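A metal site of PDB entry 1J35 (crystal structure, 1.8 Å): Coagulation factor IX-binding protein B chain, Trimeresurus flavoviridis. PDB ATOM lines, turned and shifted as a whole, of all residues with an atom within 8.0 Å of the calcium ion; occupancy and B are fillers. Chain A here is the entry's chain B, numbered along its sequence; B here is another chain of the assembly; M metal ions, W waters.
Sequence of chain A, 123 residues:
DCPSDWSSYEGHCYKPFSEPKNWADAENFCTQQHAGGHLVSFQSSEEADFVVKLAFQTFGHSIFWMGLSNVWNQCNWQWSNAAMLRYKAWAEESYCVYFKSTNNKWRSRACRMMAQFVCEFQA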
ATOM      1  N   TYR A   9      -2.990  -5.183  29.076  1.00  0.00           N
ATOM      2  CA  TYR A   9      -1.657  -4.806  28.596  1.00  0.00           C
ATOM      3  C   TYR A   9      -1.714  -4.416  27.123  1.00  0.00           C
ATOM      4  O   TYR A   9      -2.088  -5.227  26.272  1.00  0.00           O
ATOM      5  CB  TYR A   9      -0.664  -5.959  28.780  1.00  0.00           C
ATOM      6  CG  TYR A   9       0.648  -5.769  28.009  1.00  0.00           C
ATOM      7  CD1 TYR A   9       0.766  -6.163  26.668  1.00  0.00           C
ATOM      8  CD2 TYR A   9       1.756  -5.164  28.608  1.00  0.00           C
ATOM      9  CE1 TYR A   9       1.941  -5.955  25.946  1.00  0.00           C
ATOM     10  CE2 TYR A   9       2.934  -4.933  27.886  1.00  0.00           C
ATOM     11  CZ  TYR A   9       3.024  -5.333  26.556  1.00  0.00           C
ATOM     12  OH  TYR A   9       4.172  -5.084  25.839  1.00  0.00           O
ATOM     13  N   HIS A  12      -4.844  -5.038  25.025  1.00  0.00           N
ATOM     14  CA  HIS A  12      -5.230  -6.442  24.928  1.00  0.00           C
ATOM     15  C   HIS A  12      -5.543  -7.006  26.299  1.00  0.00           C
ATOM     16  O   HIS A  12      -5.112  -6.474  27.335  1.00  0.00           O
ATOM     17  CB  HIS A  12      -4.121  -7.276  24.265  1.00  0.00           C
ATOM     18  CG  HIS A  12      -4.024  -7.113  22.785  1.00  0.00           C
ATOM     19  ND1 HIS A  12      -3.359  -8.023  21.984  1.00  0.00           N
ATOM     20  CD2 HIS A  12      -4.478  -6.151  21.954  1.00  0.00           C
ATOM     21  CE1 HIS A  12      -3.419  -7.623  20.721  1.00  0.00           C
ATOM     22  NE2 HIS A  12      -4.097  -6.489  20.682  1.00  0.00           N
ATOM     23  N   CYS A  13      -6.300  -8.094  26.303  1.00  0.00           N
ATOM     24  CA  CYS A  13      -6.681  -8.747  27.542  1.00  0.00           C
ATOM     25  C   CYS A  13      -6.124 -10.165  27.559  1.00  0.00           C
ATOM     26  O   CYS A  13      -6.208 -10.883  26.566  1.00  0.00           O
ATOM     27  CB  CYS A  13      -8.203  -8.771  27.657  1.00  0.00           C
ATOM     28  SG  CYS A  13      -8.919  -7.093  27.741  1.00  0.00           S
ATOM     29  N   TYR A  14      -5.547 -10.552  28.700  1.00  0.00           N
ATOM     30  CA  TYR A  14      -4.933 -11.868  28.876  1.00  0.00           C
ATOM     31  C   TYR A  14      -5.419 -12.547  30.151  1.00  0.00           C
ATOM     32  O   TYR A  14      -5.707 -11.885  31.150  1.00  0.00           O
ATOM     33  CB  TYR A  14      -3.411 -11.721  28.962  1.00  0.00           C
ATOM     34  CG  TYR A  14      -2.787 -10.974  27.805  1.00  0.00           C
ATOM     35  CD1 TYR A  14      -2.235 -11.664  26.721  1.00  0.00           C
ATOM     36  CD2 TYR A  14      -2.788  -9.582  27.763  1.00  0.00           C
ATOM     37  CE1 TYR A  14      -1.695 -10.993  25.628  1.00  0.00           C
ATOM     38  CE2 TYR A  14      -2.261  -8.890  26.672  1.00  0.00           C
ATOM     39  CZ  TYR A  14      -1.718  -9.593  25.608  1.00  0.00           C
ATOM     40  OH  TYR A  14      -1.223  -8.916  24.530  1.00  0.00           O
ATOM     41  N   LEU A  39      -5.460 -18.593  21.810  1.00  0.00           N
ATOM     42  CA  LEU A  39      -4.340 -18.912  22.680  1.00  0.00           C
ATOM     43  C   LEU A  39      -3.411 -17.709  22.551  1.00  0.00           C
ATOM     44  O   LEU A  39      -3.354 -17.069  21.501  1.00  0.00           O
ATOM     45  CB  LEU A  39      -3.630 -20.182  22.196  1.00  0.00           C
ATOM     46  CG  LEU A  39      -4.201 -21.499  22.729  1.00  0.00           C
ATOM     47  CD1 LEU A  39      -3.504 -22.665  22.069  1.00  0.00           C
ATOM     48  CD2 LEU A  39      -4.034 -21.550  24.232  1.00  0.00           C
ATOM     49  N   VAL A  40      -2.689 -17.396  23.619  1.00  0.00           N
ATOM     50  CA  VAL A  40      -1.806 -16.232  23.622  1.00  0.00           C
ATOM     51  C   VAL A  40      -0.743 -16.261  22.518  1.00  0.00           C
ATOM     52  O   VAL A  40      -0.143 -17.297  22.248  1.00  0.00           O
ATOM     53  CB  VAL A  40      -1.132 -16.075  25.010  1.00  0.00           C
ATOM     54  CG1 VAL A  40      -0.136 -17.199  25.252  1.00  0.00           C
ATOM     55  CG2 VAL A  40      -0.461 -14.706  25.110  1.00  0.00           C
ATOM     56  N   SER A  41      -0.551 -15.107  21.866  1.00  0.00           N
ATOM     57  CA  SER A  41       0.430 -14.953  20.790  1.00  0.00           C
ATOM     58  C   SER A  41       1.474 -13.913  21.198  1.00  0.00           C
ATOM     59  O   SER A  41       1.122 -12.844  21.698  1.00  0.00           O
ATOM     60  CB  SER A  41      -0.257 -14.505  19.500  1.00  0.00           C
ATOM     61  OG  SER A  41      -1.016 -13.324  19.696  1.00  0.00           O
ATOM     62  N   PHE A  42       2.753 -14.229  21.011  1.00  0.00           N
ATOM     63  CA  PHE A  42       3.810 -13.293  21.375  1.00  0.00           C
ATOM     64  C   PHE A  42       4.362 -12.604  20.135  1.00  0.00           C
ATOM     65  O   PHE A  42       5.219 -13.158  19.442  1.00  0.00           O
ATOM     66  CB  PHE A  42       4.958 -14.023  22.114  1.00  0.00           C
ATOM     67  CG  PHE A  42       4.568 -14.598  23.472  1.00  0.00           C
ATOM     68  CD1 PHE A  42       3.413 -14.177  24.128  1.00  0.00           C
ATOM     69  CD2 PHE A  42       5.406 -15.524  24.104  1.00  0.00           C
ATOM     70  CE1 PHE A  42       3.093 -14.677  25.394  1.00  0.00           C
ATOM     71  CE2 PHE A  42       5.087 -16.038  25.366  1.00  0.00           C
ATOM     72  CZ  PHE A  42       3.930 -15.607  26.013  1.00  0.00           C
ATOM     73  N   GLN A  43       3.873 -11.402  19.850  1.00  0.00           N
ATOM     74  CA  GLN A  43       4.326 -10.646  18.688  1.00  0.00           C
ATOM     75  C   GLN A  43       5.544  -9.803  19.036  1.00  0.00           C
ATOM     76  O   GLN A  43       6.201  -9.249  18.143  1.00  0.00           O
ATOM     77  CB  GLN A  43       3.209  -9.736  18.161  1.00  0.00           C
ATOM     78  CG  GLN A  43       2.205 -10.415  17.244  1.00  0.00           C
ATOM     79  CD  GLN A  43       1.216 -11.310  17.983  1.00  0.00           C
ATOM     80  OE1 GLN A  43       1.051 -11.179  19.194  1.00  0.00           O
ATOM     81  NE2 GLN A  43       0.535 -12.188  17.253  1.00  0.00           N
ATOM     82  N   SER A  44       5.847  -9.698  20.331  1.00  0.00           N
ATOM     83  CA  SER A  44       7.009  -8.932  20.786  1.00  0.00           C
ATOM     84  C   SER A  44       7.512  -9.466  22.120  1.00  0.00           C
ATOM     85  O   SER A  44       6.789 -10.143  22.846  1.00  0.00           O
ATOM     86  CB  SER A  44       6.648  -7.438  20.933  1.00  0.00           C
ATOM     87  OG  SER A  44       5.821  -7.210  22.061  1.00  0.00           O
ATOM     88  N   GLU A  47       5.446  -8.126  25.161  1.00  0.00           N
ATOM     89  CA  GLU A  47       4.185  -8.830  25.402  1.00  0.00           C
ATOM     90  C   GLU A  47       4.471 -10.126  26.162  1.00  0.00           C
ATOM     91  O   GLU A  47       3.813 -10.439  27.142  1.00  0.00           O
ATOM     92  CB  GLU A  47       3.479  -9.162  24.081  1.00  0.00           C
ATOM     93  CG  GLU A  47       2.082  -9.770  24.246  1.00  0.00           C
ATOM     94  CD  GLU A  47       1.454 -10.168  22.923  1.00  0.00           C
ATOM     95  OE1 GLU A  47       0.258 -10.553  22.902  1.00  0.00           O
ATOM     96  OE2 GLU A  47       2.157 -10.099  21.883  1.00  0.00           O
ATOM     97  N   ALA A  48       5.476 -10.858  25.684  1.00  0.00           N
ATOM     98  CA  ALA A  48       5.861 -12.118  26.316  1.00  0.00           C
ATOM     99  C   ALA A  48       6.268 -11.868  27.763  1.00  0.00           C
ATOM    100  O   ALA A  48       5.937 -12.657  28.654  1.00  0.00           O
ATOM    101  CB  ALA A  48       7.024 -12.756  25.544  1.00  0.00           C
ATOM    102  N   VAL A  51       2.999 -11.523  29.819  1.00  0.00           N
ATOM    103  CA  VAL A  51       2.347 -12.820  29.977  1.00  0.00           C
ATOM    104  C   VAL A  51       3.070 -13.804  30.899  1.00  0.00           C
ATOM    105  O   VAL A  51       2.447 -14.421  31.762  1.00  0.00           O
ATOM    106  CB  VAL A  51       2.137 -13.497  28.599  1.00  0.00           C
ATOM    107  CG1 VAL A  51       1.415 -14.833  28.772  1.00  0.00           C
ATOM    108  CG2 VAL A  51       1.335 -12.569  27.698  1.00  0.00           C
ATOM    109  N   GLU A 120      -6.119 -14.799  24.979  1.00  0.00           N
ATOM    110  CA  GLU A 120      -5.917 -13.390  24.668  1.00  0.00           C
ATOM    111  C   GLU A 120      -6.888 -12.921  23.591  1.00  0.00           C
ATOM    112  O   GLU A 120      -7.316 -13.711  22.753  1.00  0.00           O
ATOM    113  CB  GLU A 120      -4.470 -13.182  24.147  1.00  0.00           C
ATOM    114  CG  GLU A 120      -4.201 -11.814  23.519  1.00  0.00           C
ATOM    115  CD  GLU A 120      -2.920 -11.771  22.680  1.00  0.00           C
ATOM    116  OE1 GLU A 120      -2.619 -10.705  22.089  1.00  0.00           O
ATOM    117  OE2 GLU A 120      -2.222 -12.794  22.584  1.00  0.00           O
ATOM    118  N   PHE A 121      -7.241 -11.642  23.635  1.00  0.00           N
ATOM    119  CA  PHE A 121      -8.115 -11.037  22.632  1.00  0.00           C
ATOM    120  C   PHE A 121      -7.873  -9.529  22.591  1.00  0.00           C
ATOM    121  O   PHE A 121      -7.447  -8.936  23.588  1.00  0.00           O
ATOM    122  CB  PHE A 121      -9.590 -11.334  22.900  1.00  0.00           C
ATOM    123  CG  PHE A 121     -10.164 -10.638  24.115  1.00  0.00           C
ATOM    124  CD1 PHE A 121     -10.150 -11.265  25.363  1.00  0.00           C
ATOM    125  CD2 PHE A 121     -10.758  -9.382  24.006  1.00  0.00           C
ATOM    126  CE1 PHE A 121     -10.724 -10.660  26.479  1.00  0.00           C
ATOM    127  CE2 PHE A 121     -11.340  -8.762  25.118  1.00  0.00           C
ATOM    128  CZ  PHE A 121     -11.325  -9.403  26.363  1.00  0.00           C
ATOM    129  N   GLN A 122      -8.132  -8.913  21.445  1.00  0.00           N
ATOM    130  CA  GLN A 122      -7.940  -7.473  21.288  1.00  0.00           C
ATOM    131  C   GLN A 122      -9.179  -6.729  21.779  1.00  0.00           C
ATOM    132  O   GLN A 122     -10.282  -6.944  21.263  1.00  0.00           O
ATOM    133  CB  GLN A 122      -7.663  -7.130  19.826  1.00  0.00           C
ATOM    134  CG  GLN A 122      -7.401  -5.646  19.556  1.00  0.00           C
ATOM    135  CD  GLN A 122      -6.757  -5.396  18.205  1.00  0.00           C
ATOM    136  OE1 GLN A 122      -5.641  -5.837  17.939  1.00  0.00           O
ATOM    137  NE2 GLN A 122      -7.468  -4.673  17.333  1.00  0.00           N
ATOM    138  N   TRP B  83       0.089 -17.601  13.789  1.00  0.00           N
ATOM    139  CA  TRP B  83      -0.549 -17.583  15.103  1.00  0.00           C
ATOM    140  C   TRP B  83      -2.014 -17.929  14.898  1.00  0.00           C
ATOM    141  O   TRP B  83      -2.599 -17.585  13.866  1.00  0.00           O
ATOM    142  CB  TRP B  83      -0.431 -16.203  15.747  1.00  0.00           C
ATOM    143  CG  TRP B  83       0.970 -15.794  16.078  1.00  0.00           C
ATOM    144  CD1 TRP B  83       1.755 -14.916  15.388  1.00  0.00           C
ATOM    145  CD2 TRP B  83       1.738 -16.233  17.198  1.00  0.00           C
ATOM    146  NE1 TRP B  83       2.961 -14.780  16.015  1.00  0.00           N
ATOM    147  CE2 TRP B  83       2.988 -15.585  17.135  1.00  0.00           C
ATOM    148  CE3 TRP B  83       1.500 -17.126  18.258  1.00  0.00           C
ATOM    149  CZ2 TRP B  83       3.996 -15.786  18.075  1.00  0.00           C
ATOM    150  CZ3 TRP B  83       2.501 -17.326  19.192  1.00  0.00           C
ATOM    151  CH2 TRP B  83       3.734 -16.655  19.094  1.00  0.00           C
ATOM    152  N   ASP B  85      -4.472 -16.609  16.052  1.00  0.00           N
ATOM    153  CA  ASP B  85      -5.255 -15.389  15.878  1.00  0.00           C
ATOM    154  C   ASP B  85      -5.299 -14.956  14.414  1.00  0.00           C
ATOM    155  O   ASP B  85      -6.080 -14.082  14.050  1.00  0.00           O
ATOM    156  CB  ASP B  85      -4.683 -14.256  16.743  1.00  0.00           C
ATOM    157  CG  ASP B  85      -3.332 -13.754  16.242  1.00  0.00           C
ATOM    158  OD1 ASP B  85      -2.730 -12.922  16.954  1.00  0.00           O
ATOM    159  OD2 ASP B  85      -2.876 -14.166  15.162  1.00  0.00           O
ATOM    160  N   SER B  87      -2.500 -13.843  12.654  1.00  0.00           N
ATOM    161  CA  SER B  87      -1.353 -13.003  12.310  1.00  0.00           C
ATOM    162  C   SER B  87      -0.106 -13.804  11.951  1.00  0.00           C
ATOM    163  O   SER B  87       0.039 -14.980  12.327  1.00  0.00           O
ATOM    164  CB  SER B  87      -1.022 -12.063  13.459  1.00  0.00           C
ATOM    165  OG  SER B  87      -0.520 -12.786  14.566  1.00  0.00           O
HETATM  166 CA    CA M   1      -0.562 -11.218  21.005  1.00  0.00          CA
HETATM  167  O   HOH W   1      -0.504  -8.963  20.806  1.00  0.00           O
HETATM  168  O   HOH W   2      -2.368 -11.197  19.325  1.00  0.00           O
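OH of Tyr 9 is in hydrogen-bond range of N of Glu 47 (3.4 Å).
The side-chain amide nitrogen (NE2) of Gln 43 lies within hydrogen-bond range of the side-chain hydroxyl (OG) of Ser 87 of chain B (2.9 Å).
ND1 of His 12 sits close to OE1 of Glu 120 (2.8 Å).
OG of Ser 41 lies close to OD1 of Asp 85 of chain B (3.3 Å).
The side-chain hydroxyl (OH) of Tyr 14 sits close to the side-chain carboxylate (OE1) of Glu 120.
The side-chain hydroxyl (OH) of Tyr 14 lies close to the side-chain carboxylate (OE1) of Glu 47, at 2.7 Å.
The side-chain hydroxyl (OG) of Ser 44 sits at hydrogen-bond distance from the backbone NH (N) of Glu 47 (3.3 Å).
The side-chain carboxylate of Asp 85 of chain B is in hydrogen-bond range of the side-chain amide nitrogen of Gln 43, at 3.4 Å.
Of the 19 residues printed, 4 come within 4 Å of the calcium ion.
The nearest printed residue that does not touch the calcium ion is Tyr 14 (4.3 Å).
The calcium ion is bound by OE1 of Glu 47, water W1, OE1 of Glu 120, OE1 of Gln 43, O of Ser 41, water W2, OG of Ser 41 and OE2 of Glu 120.
Slightly farther from the calcium ion lies the side-chain carboxylate (OE2) of Glu 47 (3.1 Å).
Water W1 bridges the side-chain carboxylate of Glu 47 and a ring nitrogen (ND1) of His 12.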
